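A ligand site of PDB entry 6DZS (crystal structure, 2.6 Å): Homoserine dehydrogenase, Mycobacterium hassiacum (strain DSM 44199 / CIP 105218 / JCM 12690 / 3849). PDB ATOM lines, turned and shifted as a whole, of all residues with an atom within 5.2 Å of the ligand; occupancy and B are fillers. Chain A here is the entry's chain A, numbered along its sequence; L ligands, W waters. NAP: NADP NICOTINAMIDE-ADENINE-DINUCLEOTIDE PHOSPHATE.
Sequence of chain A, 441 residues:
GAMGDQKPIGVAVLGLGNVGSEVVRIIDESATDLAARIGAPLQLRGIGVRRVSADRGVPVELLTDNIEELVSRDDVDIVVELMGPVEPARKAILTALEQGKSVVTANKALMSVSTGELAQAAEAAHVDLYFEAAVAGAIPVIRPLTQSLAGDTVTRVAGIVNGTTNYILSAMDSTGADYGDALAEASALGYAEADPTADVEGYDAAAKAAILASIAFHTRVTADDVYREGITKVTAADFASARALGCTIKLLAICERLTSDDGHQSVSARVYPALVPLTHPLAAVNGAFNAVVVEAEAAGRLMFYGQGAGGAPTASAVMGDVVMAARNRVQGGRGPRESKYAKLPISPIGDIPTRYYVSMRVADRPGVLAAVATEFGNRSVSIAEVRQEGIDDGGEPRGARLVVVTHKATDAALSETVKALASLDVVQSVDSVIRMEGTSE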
ATOM      1  N   LEU A  14      -6.744   8.350   7.601  1.00  0.00           N
ATOM      2  CA  LEU A  14      -7.958   9.119   7.372  1.00  0.00           C
ATOM      3  C   LEU A  14      -7.623  10.253   6.415  1.00  0.00           C
ATOM      4  O   LEU A  14      -6.947  11.211   6.796  1.00  0.00           O
ATOM      5  CB  LEU A  14      -8.521   9.652   8.682  1.00  0.00           C
ATOM      6  CG  LEU A  14      -8.660   8.616   9.790  1.00  0.00           C
ATOM      7  CD1 LEU A  14      -9.228   9.273  11.035  1.00  0.00           C
ATOM      8  CD2 LEU A  14      -9.527   7.445   9.337  1.00  0.00           C
ATOM      9  N   GLY A  15      -8.102  10.143   5.191  1.00  0.00           N
ATOM     10  CA  GLY A  15      -7.812  11.133   4.170  1.00  0.00           C
ATOM     11  C   GLY A  15      -6.907  10.557   3.112  1.00  0.00           C
ATOM     12  O   GLY A  15      -5.944   9.825   3.404  1.00  0.00           O
ATOM     13  N   LEU A  16      -7.214  10.873   1.852  1.00  0.00           N
ATOM     14  CA  LEU A  16      -6.446  10.409   0.706  1.00  0.00           C
ATOM     15  C   LEU A  16      -6.212  11.569  -0.245  1.00  0.00           C
ATOM     16  O   LEU A  16      -6.229  11.411  -1.469  1.00  0.00           O
ATOM     17  CB  LEU A  16      -7.153   9.255   0.009  1.00  0.00           C
ATOM     18  CG  LEU A  16      -6.295   8.395  -0.918  1.00  0.00           C
ATOM     19  CD1 LEU A  16      -5.254   7.608  -0.129  1.00  0.00           C
ATOM     20  CD2 LEU A  16      -7.168   7.450  -1.729  1.00  0.00           C
ATOM     21  N   GLY A  17      -5.998  12.755   0.314  1.00  0.00           N
ATOM     22  CA  GLY A  17      -5.749  13.945  -0.467  1.00  0.00           C
ATOM     23  C   GLY A  17      -4.277  14.174  -0.741  1.00  0.00           C
ATOM     24  O   GLY A  17      -3.533  13.227  -1.030  1.00  0.00           O
ATOM     25  N   ASN A  18      -3.823  15.434  -0.645  1.00  0.00           N
ATOM     26  CA  ASN A  18      -2.438  15.746  -0.965  1.00  0.00           C
ATOM     27  C   ASN A  18      -1.475  14.978  -0.065  1.00  0.00           C
ATOM     28  O   ASN A  18      -0.494  14.405  -0.541  1.00  0.00           O
ATOM     29  CB  ASN A  18      -2.200  17.250  -0.848  1.00  0.00           C
ATOM     30  CG  ASN A  18      -2.955  18.045  -1.891  1.00  0.00           C
ATOM     31  OD1 ASN A  18      -2.713  17.902  -3.088  1.00  0.00           O
ATOM     32  ND2 ASN A  18      -3.883  18.879  -1.447  1.00  0.00           N
ATOM     33  N   VAL A  19      -1.739  14.978   1.236  1.00  0.00           N
ATOM     34  CA  VAL A  19      -0.846  14.314   2.195  1.00  0.00           C
ATOM     35  C   VAL A  19      -1.161  12.836   2.303  1.00  0.00           C
ATOM     36  O   VAL A  19      -0.262  11.995   2.212  1.00  0.00           O
ATOM     37  CB  VAL A  19      -0.929  15.020   3.564  1.00  0.00           C
ATOM     38  CG1 VAL A  19       0.007  14.355   4.566  1.00  0.00           C
ATOM     39  CG2 VAL A  19      -0.591  16.483   3.431  1.00  0.00           C
ATOM     40  N   GLY A  20      -2.434  12.483   2.507  1.00  0.00           N
ATOM     41  CA  GLY A  20      -2.788  11.096   2.719  1.00  0.00           C
ATOM     42  C   GLY A  20      -2.401  10.194   1.566  1.00  0.00           C
ATOM     43  O   GLY A  20      -1.954   9.064   1.763  1.00  0.00           O
ATOM     44  N   GLY A  48      -9.774   6.055   5.300  1.00  0.00           N
ATOM     45  CA  GLY A  48     -10.960   6.873   5.452  1.00  0.00           C
ATOM     46  C   GLY A  48     -11.009   7.943   4.378  1.00  0.00           C
ATOM     47  O   GLY A  48     -10.027   8.595   4.077  1.00  0.00           O
ATOM     48  N   VAL A  49     -12.199   8.108   3.787  1.00  0.00           N
ATOM     49  CA  VAL A  49     -12.399   9.036   2.686  1.00  0.00           C
ATOM     50  C   VAL A  49     -13.869   9.423   2.704  1.00  0.00           C
ATOM     51  O   VAL A  49     -14.644   8.903   3.511  1.00  0.00           O
ATOM     52  CB  VAL A  49     -11.995   8.391   1.349  1.00  0.00           C
ATOM     53  CG1 VAL A  49     -12.971   7.274   0.954  1.00  0.00           C
ATOM     54  CG2 VAL A  49     -11.863   9.426   0.236  1.00  0.00           C
ATOM     55  N   ARG A  50     -14.266  10.357   1.837  1.00  0.00           N
ATOM     56  CA  ARG A  50     -15.666  10.635   1.582  1.00  0.00           C
ATOM     57  C   ARG A  50     -16.164   9.974   0.301  1.00  0.00           C
ATOM     58  O   ARG A  50     -17.158   9.243   0.327  1.00  0.00           O
ATOM     59  CB  ARG A  50     -15.904  12.145   1.530  1.00  0.00           C
ATOM     60  CG  ARG A  50     -15.760  12.817   2.882  1.00  0.00           C
ATOM     61  CD  ARG A  50     -16.032  14.308   2.814  1.00  0.00           C
ATOM     62  NE  ARG A  50     -15.047  15.006   1.997  1.00  0.00           N
ATOM     63  CZ  ARG A  50     -14.909  16.323   1.952  1.00  0.00           C
ATOM     64  NH1 ARG A  50     -15.693  17.104   2.691  1.00  0.00           N
ATOM     65  NH2 ARG A  50     -13.983  16.871   1.173  1.00  0.00           N
ATOM     66  N   ARG A  51     -15.477  10.201  -0.819  1.00  0.00           N
ATOM     67  CA  ARG A  51     -15.797   9.523  -2.074  1.00  0.00           C
ATOM     68  C   ARG A  51     -15.106   8.173  -2.123  1.00  0.00           C
ATOM     69  O   ARG A  51     -13.891   8.077  -1.951  1.00  0.00           O
ATOM     70  CB  ARG A  51     -15.357  10.370  -3.279  1.00  0.00           C
ATOM     71  CG  ARG A  51     -16.189  11.629  -3.502  1.00  0.00           C
ATOM     72  CD  ARG A  51     -15.813  12.329  -4.811  1.00  0.00           C
ATOM     73  NE  ARG A  51     -14.426  12.829  -4.826  1.00  0.00           N
ATOM     74  CZ  ARG A  51     -13.412  12.260  -5.478  1.00  0.00           C
ATOM     75  NH1 ARG A  51     -13.592  11.160  -6.206  1.00  0.00           N
ATOM     76  NH2 ARG A  51     -12.205  12.816  -5.410  1.00  0.00           N
ATOM     77  N   ARG A  56      -8.798   5.926  -7.427  1.00  0.00           N
ATOM     78  CA  ARG A  56      -8.056   6.646  -6.395  1.00  0.00           C
ATOM     79  C   ARG A  56      -6.732   5.964  -6.069  1.00  0.00           C
ATOM     80  O   ARG A  56      -6.233   6.052  -4.947  1.00  0.00           O
ATOM     81  CB  ARG A  56      -8.903   6.797  -5.135  1.00  0.00           C
ATOM     82  CG  ARG A  56     -10.208   7.543  -5.372  1.00  0.00           C
ATOM     83  CD  ARG A  56     -10.932   7.787  -4.065  1.00  0.00           C
ATOM     84  NE  ARG A  56     -10.220   8.742  -3.232  1.00  0.00           N
ATOM     85  CZ  ARG A  56     -10.568  10.022  -3.073  1.00  0.00           C
ATOM     86  NH1 ARG A  56     -11.632  10.520  -3.677  1.00  0.00           N
ATOM     87  NH2 ARG A  56      -9.835  10.809  -2.298  1.00  0.00           N
ATOM     88  N   ILE A  67     -15.808   6.490   9.174  1.00  0.00           N
ATOM     89  CA  ILE A  67     -14.547   6.754   9.858  1.00  0.00           C
ATOM     90  C   ILE A  67     -14.550   6.138  11.242  1.00  0.00           C
ATOM     91  O   ILE A  67     -13.530   5.622  11.710  1.00  0.00           O
ATOM     92  CB  ILE A  67     -14.278   8.267   9.899  1.00  0.00           C
ATOM     93  CG1 ILE A  67     -14.302   8.857   8.490  1.00  0.00           C
ATOM     94  CG2 ILE A  67     -12.944   8.560  10.580  1.00  0.00           C
ATOM     95  CD1 ILE A  67     -13.343   8.179   7.512  1.00  0.00           C
ATOM     96  N   GLU A  81      -4.640  10.911  11.130  1.00  0.00           N
ATOM     97  CA  GLU A  81      -5.687  11.871  10.762  1.00  0.00           C
ATOM     98  C   GLU A  81      -5.101  12.864   9.756  1.00  0.00           C
ATOM     99  O   GLU A  81      -4.253  13.682  10.107  1.00  0.00           O
ATOM    100  CB  GLU A  81      -6.221  12.589  11.995  1.00  0.00           C
ATOM    101  CG  GLU A  81      -7.470  13.432  11.756  1.00  0.00           C
ATOM    102  CD  GLU A  81      -7.175  14.765  11.088  1.00  0.00           C
ATOM    103  OE1 GLU A  81      -6.196  15.439  11.479  1.00  0.00           O
ATOM    104  OE2 GLU A  81      -7.929  15.144  10.169  1.00  0.00           O
ATOM    105  N   LEU A  82      -5.576  12.786   8.517  1.00  0.00           N
ATOM    106  CA  LEU A  82      -5.160  13.696   7.457  1.00  0.00           C
ATOM    107  C   LEU A  82      -6.371  14.212   6.688  1.00  0.00           C
ATOM    108  O   LEU A  82      -6.281  14.474   5.480  1.00  0.00           O
ATOM    109  CB  LEU A  82      -4.159  13.017   6.523  1.00  0.00           C
ATOM    110  CG  LEU A  82      -2.843  12.623   7.219  1.00  0.00           C
ATOM    111  CD1 LEU A  82      -2.006  11.726   6.331  1.00  0.00           C
ATOM    112  CD2 LEU A  82      -2.040  13.851   7.637  1.00  0.00           C
ATOM    113  N   MET A  83      -7.503  14.347   7.374  1.00  0.00           N
ATOM    114  CA  MET A  83      -8.664  15.035   6.853  1.00  0.00           C
ATOM    115  C   MET A  83      -8.553  16.520   7.188  1.00  0.00           C
ATOM    116  O   MET A  83      -7.886  16.903   8.155  1.00  0.00           O
ATOM    117  CB  MET A  83      -9.961  14.479   7.448  1.00  0.00           C
ATOM    118  CG  MET A  83     -10.091  12.971   7.409  1.00  0.00           C
ATOM    119  SD  MET A  83     -11.583  12.431   8.267  1.00  0.00           S
ATOM    120  CE  MET A  83     -11.154  12.722   9.982  1.00  0.00           C
ATOM    121  N   GLY A  84      -9.204  17.345   6.401  1.00  0.00           N
ATOM    122  CA  GLY A  84      -9.192  18.767   6.651  1.00  0.00           C
ATOM    123  C   GLY A  84      -9.949  19.138   7.911  1.00  0.00           C
ATOM    124  O   GLY A  84      -9.365  19.528   8.932  1.00  0.00           O
ATOM    125  N   PRO A  85     -11.276  19.016   7.849  1.00  0.00           N
ATOM    126  CA  PRO A  85     -12.133  19.637   8.864  1.00  0.00           C
ATOM    127  C   PRO A  85     -11.747  19.284  10.298  1.00  0.00           C
ATOM    128  O   PRO A  85     -11.227  18.202  10.571  1.00  0.00           O
ATOM    129  CB  PRO A  85     -13.526  19.103   8.515  1.00  0.00           C
ATOM    130  CG  PRO A  85     -13.447  18.843   7.050  1.00  0.00           C
ATOM    131  CD  PRO A  85     -12.047  18.362   6.786  1.00  0.00           C
ATOM    132  N   PRO A  88     -14.891  16.790  12.400  1.00  0.00           N
ATOM    133  CA  PRO A  88     -14.613  15.371  12.123  1.00  0.00           C
ATOM    134  C   PRO A  88     -13.259  14.940  12.651  1.00  0.00           C
ATOM    135  O   PRO A  88     -13.124  13.824  13.163  1.00  0.00           O
ATOM    136  CB  PRO A  88     -14.665  15.296  10.589  1.00  0.00           C
ATOM    137  CG  PRO A  88     -15.459  16.467  10.162  1.00  0.00           C
ATOM    138  CD  PRO A  88     -15.190  17.542  11.164  1.00  0.00           C
ATOM    139  N   ALA A 106      -1.663  15.986  11.314  1.00  0.00           N
ATOM    140  CA  ALA A 106      -0.983  17.146  10.750  1.00  0.00           C
ATOM    141  C   ALA A 106      -1.870  18.383  10.821  1.00  0.00           C
ATOM    142  O   ALA A 106      -1.630  19.353  10.086  1.00  0.00           O
ATOM    143  CB  ALA A 106      -0.560  16.880   9.308  1.00  0.00           C
ATOM    144  N   ASN A 107      -2.873  18.381  11.698  1.00  0.00           N
ATOM    145  CA  ASN A 107      -3.953  19.365  11.663  1.00  0.00           C
ATOM    146  C   ASN A 107      -3.534  20.619  12.435  1.00  0.00           C
ATOM    147  O   ASN A 107      -3.597  20.662  13.665  1.00  0.00           O
ATOM    148  CB  ASN A 107      -5.213  18.748  12.246  1.00  0.00           C
ATOM    149  CG  ASN A 107      -6.454  19.543  11.928  1.00  0.00           C
ATOM    150  OD1 ASN A 107      -6.451  20.771  12.016  1.00  0.00           O
ATOM    151  ND2 ASN A 107      -7.525  18.856  11.542  1.00  0.00           N
ATOM    152  N   LYS A 108      -3.097  21.649  11.692  1.00  0.00           N
ATOM    153  CA  LYS A 108      -2.692  22.903  12.317  1.00  0.00           C
ATOM    154  C   LYS A 108      -3.800  23.474  13.189  1.00  0.00           C
ATOM    155  O   LYS A 108      -3.569  23.821  14.346  1.00  0.00           O
ATOM    156  CB  LYS A 108      -2.316  23.927  11.240  1.00  0.00           C
ATOM    157  CG  LYS A 108      -1.142  23.559  10.371  1.00  0.00           C
ATOM    158  CD  LYS A 108      -0.940  24.561   9.227  1.00  0.00           C
ATOM    159  CE  LYS A 108      -2.018  24.427   8.151  1.00  0.00           C
ATOM    160  NZ  LYS A 108      -2.006  23.085   7.498  1.00  0.00           N
ATOM    161  N   ALA A 133       3.893  16.994  11.814  1.00  0.00           N
ATOM    162  CA  ALA A 133       3.531  17.484  10.489  1.00  0.00           C
ATOM    163  C   ALA A 133       2.667  18.738  10.543  1.00  0.00           C
ATOM    164  O   ALA A 133       2.433  19.346   9.499  1.00  0.00           O
ATOM    165  CB  ALA A 133       2.800  16.388   9.724  1.00  0.00           C
ATOM    166  N   ALA A 134       2.203  19.134  11.733  1.00  0.00           N
ATOM    167  CA  ALA A 134       1.353  20.307  11.842  1.00  0.00           C
ATOM    168  C   ALA A 134       2.132  21.598  11.592  1.00  0.00           C
ATOM    169  O   ALA A 134       1.563  22.571  11.084  1.00  0.00           O
ATOM    170  CB  ALA A 134       0.711  20.364  13.231  1.00  0.00           C
ATOM    171  N   ALA A 309       5.543  22.971   3.450  1.00  0.00           N
ATOM    172  CA  ALA A 309       4.227  22.742   2.859  1.00  0.00           C
ATOM    173  C   ALA A 309       4.396  21.785   1.687  1.00  0.00           C
ATOM    174  O   ALA A 309       5.488  21.667   1.113  1.00  0.00           O
ATOM    175  CB  ALA A 309       3.571  24.053   2.411  1.00  0.00           C
ATOM    176  N   GLY A 310       3.315  21.104   1.346  1.00  0.00           N
ATOM    177  CA  GLY A 310       3.307  20.160   0.249  1.00  0.00           C
ATOM    178  C   GLY A 310       3.016  18.742   0.688  1.00  0.00           C
ATOM    179  O   GLY A 310       3.307  18.372   1.836  1.00  0.00           O
ATOM    180  N   GLY A 311       2.442  17.937  -0.202  1.00  0.00           N
ATOM    181  CA  GLY A 311       2.078  16.585   0.162  1.00  0.00           C
ATOM    182  C   GLY A 311       3.283  15.747   0.557  1.00  0.00           C
ATOM    183  O   GLY A 311       3.280  15.078   1.592  1.00  0.00           O
ATOM    184  N   THR A 314       5.236  17.086   3.904  1.00  0.00           N
ATOM    185  CA  THR A 314       4.382  16.836   5.062  1.00  0.00           C
ATOM    186  C   THR A 314       4.297  15.350   5.374  1.00  0.00           C
ATOM    187  O   THR A 314       4.393  14.941   6.535  1.00  0.00           O
ATOM    188  CB  THR A 314       2.988  17.415   4.825  1.00  0.00           C
ATOM    189  OG1 THR A 314       3.092  18.814   4.483  1.00  0.00           O
ATOM    190  CG2 THR A 314       2.115  17.282   6.056  1.00  0.00           C
HETATM  191  PA  NAP L   1      -7.090  17.391   1.061  1.00  0.00           P
HETATM  192  O1A NAP L   1      -6.265  17.460  -0.156  1.00  0.00           O
HETATM  193  O2A NAP L   1      -8.231  18.402   0.963  1.00  0.00           O
HETATM  194  O5B NAP L   1      -7.693  15.896   1.346  1.00  0.00           O
HETATM  195  C5B NAP L   1      -8.483  15.642   2.523  1.00  0.00           C
HETATM  196  C4B NAP L   1      -8.837  14.177   2.544  1.00  0.00           C
HETATM  197  O4B NAP L   1      -9.662  13.903   3.705  1.00  0.00           O
HETATM  198  C3B NAP L   1      -9.619  13.679   1.330  1.00  0.00           C
HETATM  199  O3B NAP L   1      -9.200  12.371   0.955  1.00  0.00           O
HETATM  200  C2B NAP L   1     -11.060  13.678   1.826  1.00  0.00           C
HETATM  201  O2B NAP L   1     -11.864  12.717   1.113  1.00  0.00           O
HETATM  202  C1B NAP L   1     -10.911  13.356   3.308  1.00  0.00           C
HETATM  203  N9A NAP L   1     -11.951  13.934   4.156  1.00  0.00           N
HETATM  204  C8A NAP L   1     -12.240  15.260   4.342  1.00  0.00           C
HETATM  205  N7A NAP L   1     -13.209  15.484   5.190  1.00  0.00           N
HETATM  206  C5A NAP L   1     -13.596  14.217   5.592  1.00  0.00           C
HETATM  207  C6A NAP L   1     -14.584  13.765   6.471  1.00  0.00           C
HETATM  208  N6A NAP L   1     -15.404  14.569   7.151  1.00  0.00           N
HETATM  209  N1A NAP L   1     -14.723  12.434   6.639  1.00  0.00           N
HETATM  210  C2A NAP L   1     -13.914  11.616   5.961  1.00  0.00           C
HETATM  211  N3A NAP L   1     -12.936  11.921   5.106  1.00  0.00           N
HETATM  212  C4A NAP L   1     -12.825  13.255   4.957  1.00  0.00           C
HETATM  213  O3  NAP L   1      -6.215  17.767   2.341  1.00  0.00           O
HETATM  214  PN  NAP L   1      -4.640  17.668   2.599  1.00  0.00           P
HETATM  215  O1N NAP L   1      -3.964  18.699   1.780  1.00  0.00           O
HETATM  216  O2N NAP L   1      -4.235  16.247   2.440  1.00  0.00           O
HETATM  217  O5D NAP L   1      -4.571  18.099   4.120  1.00  0.00           O
HETATM  218  C5D NAP L   1      -4.771  17.111   5.157  1.00  0.00           C
HETATM  219  C4D NAP L   1      -4.359  17.707   6.486  1.00  0.00           C
HETATM  220  O4D NAP L   1      -2.943  17.999   6.448  1.00  0.00           O
HETATM  221  C3D NAP L   1      -5.073  19.012   6.861  1.00  0.00           C
HETATM  222  O3D NAP L   1      -5.413  19.011   8.244  1.00  0.00           O
HETATM  223  C2D NAP L   1      -4.020  20.074   6.560  1.00  0.00           C
HETATM  224  O2D NAP L   1      -4.159  21.214   7.404  1.00  0.00           O
HETATM  225  C1D NAP L   1      -2.741  19.309   6.886  1.00  0.00           C
HETATM  226  N1N NAP L   1      -1.475  19.858   6.217  1.00  0.00           N
HETATM  227  C2N NAP L   1      -1.442  19.872   4.877  1.00  0.00           C
HETATM  228  C3N NAP L   1      -0.346  20.398   4.218  1.00  0.00           C
HETATM  229  C7N NAP L   1      -0.295  20.482   2.717  1.00  0.00           C
HETATM  230  O7N NAP L   1       0.703  20.969   2.179  1.00  0.00           O
HETATM  231  N7N NAP L   1      -1.325  20.040   2.038  1.00  0.00           N
HETATM  232  C4N NAP L   1       0.711  20.886   4.964  1.00  0.00           C
HETATM  233  C5N NAP L   1       0.651  20.854   6.344  1.00  0.00           C
HETATM  234  C6N NAP L   1      -0.451  20.328   6.961  1.00  0.00           C
HETATM  235  P2B NAP L   1     -12.428  13.056  -0.353  1.00  0.00           P
HETATM  236  O1X NAP L   1     -11.321  13.200  -1.325  1.00  0.00           O
HETATM  237  O2X NAP L   1     -13.353  11.909  -0.705  1.00  0.00           O
HETATM  238  O3X NAP L   1     -13.233  14.342  -0.187  1.00  0.00           O
HETATM  239  O   HOH W   1      -0.614  20.780  -1.025  1.00  0.00           O
HETATM  240  O   HOH W   2      -4.855  21.475   1.837  1.00  0.00           O
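The backbone NH (N) of Arg 50 sits at hydrogen-bond distance from an oxygen (O2X) of the ligand (3.1 Å). The side-chain amino group (NZ) of Lys 108 is in hydrogen-bond range of an oxygen (O2D) of the ligand, at 2.9 Å. The side-chain amide nitrogen (ND2) of Asn 18 is in hydrogen-bond range of an oxygen (O1A) of the ligand. An oxygen (O3B) of the ligand sits at hydrogen-bond distance from the backbone NH of Gly 17 (3.3 Å). The backbone carbonyl oxygen of Met 83 lies within hydrogen-bond range of an oxygen (O3D) of the ligand, 3.3 Å away. The guanidinium group of Arg 56 lies within salt-bridge range of an oxygen (O1X) of the ligand (3.0 Å). An oxygen (O7N) of the ligand lies within hydrogen-bond range of the backbone NH (N) of Gly 310 (2.7 Å). O3X of the ligand is in salt-bridge range of NE of Arg 50 (2.9 Å). The backbone NH (N) of Val 19 lies within hydrogen-bond range of an oxygen (O2N) of the ligand, at 3.0 Å. The backbone NH (N) of Asn 18 is in hydrogen-bond range of an oxygen (O1A) of the ligand (3.2 Å). N of Leu 16 lies within hydrogen-bond range of O3B of the ligand. An oxygen (O2X) of the ligand is in hydrogen-bond range of the backbone NH of Arg 51 (2.7 Å).
Residues that only touch the ligand: Gly 15 (3.4 Å), Val 49 (3.0 Å), Ile 67 (3.8 Å), Leu 82 (3.1 Å), Pro 85 (3.5 Å), Pro 88 (3.6 Å), Ala 106 (3.4 Å), Asn 107 (3.7 Å), Ala 133 (3.9 Å), Ala 309 (3.8 Å) and Thr 314 (3.2 Å). Hydrophobic or aromatic side chains that line the ligand: Leu 16, Val 19, Val 49, Ile 67, Met 83, Pro 85, Pro 88 and Ala 106. The nearest printed residue that does not touch the ligand is Gly 84 (4.04 Å).
The backbone carbonyl oxygen of Leu 14 lies within hydrogen-bond range of the backbone NH of Met 83 (3.2 Å). The backbone carbonyl oxygen of Gly 84 is in hydrogen-bond range of the side-chain amide nitrogen of Asn 107, 3.3 Å away. The side-chain carboxylate (OE2) of Glu 81 sits at hydrogen-bond distance from the backbone NH (N) of Met 83. O of Gly 310 lies within hydrogen-bond range of OG1 of Thr 314 (2.7 Å). The backbone NH (N) of Gly 15 is in hydrogen-bond range of the backbone carbonyl oxygen (O) of Gly 48 (2.7 Å). The backbone NH (N) of Leu 82 lies within hydrogen-bond range of the backbone carbonyl oxygen (O) of Leu 14, at 2.7 Å.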
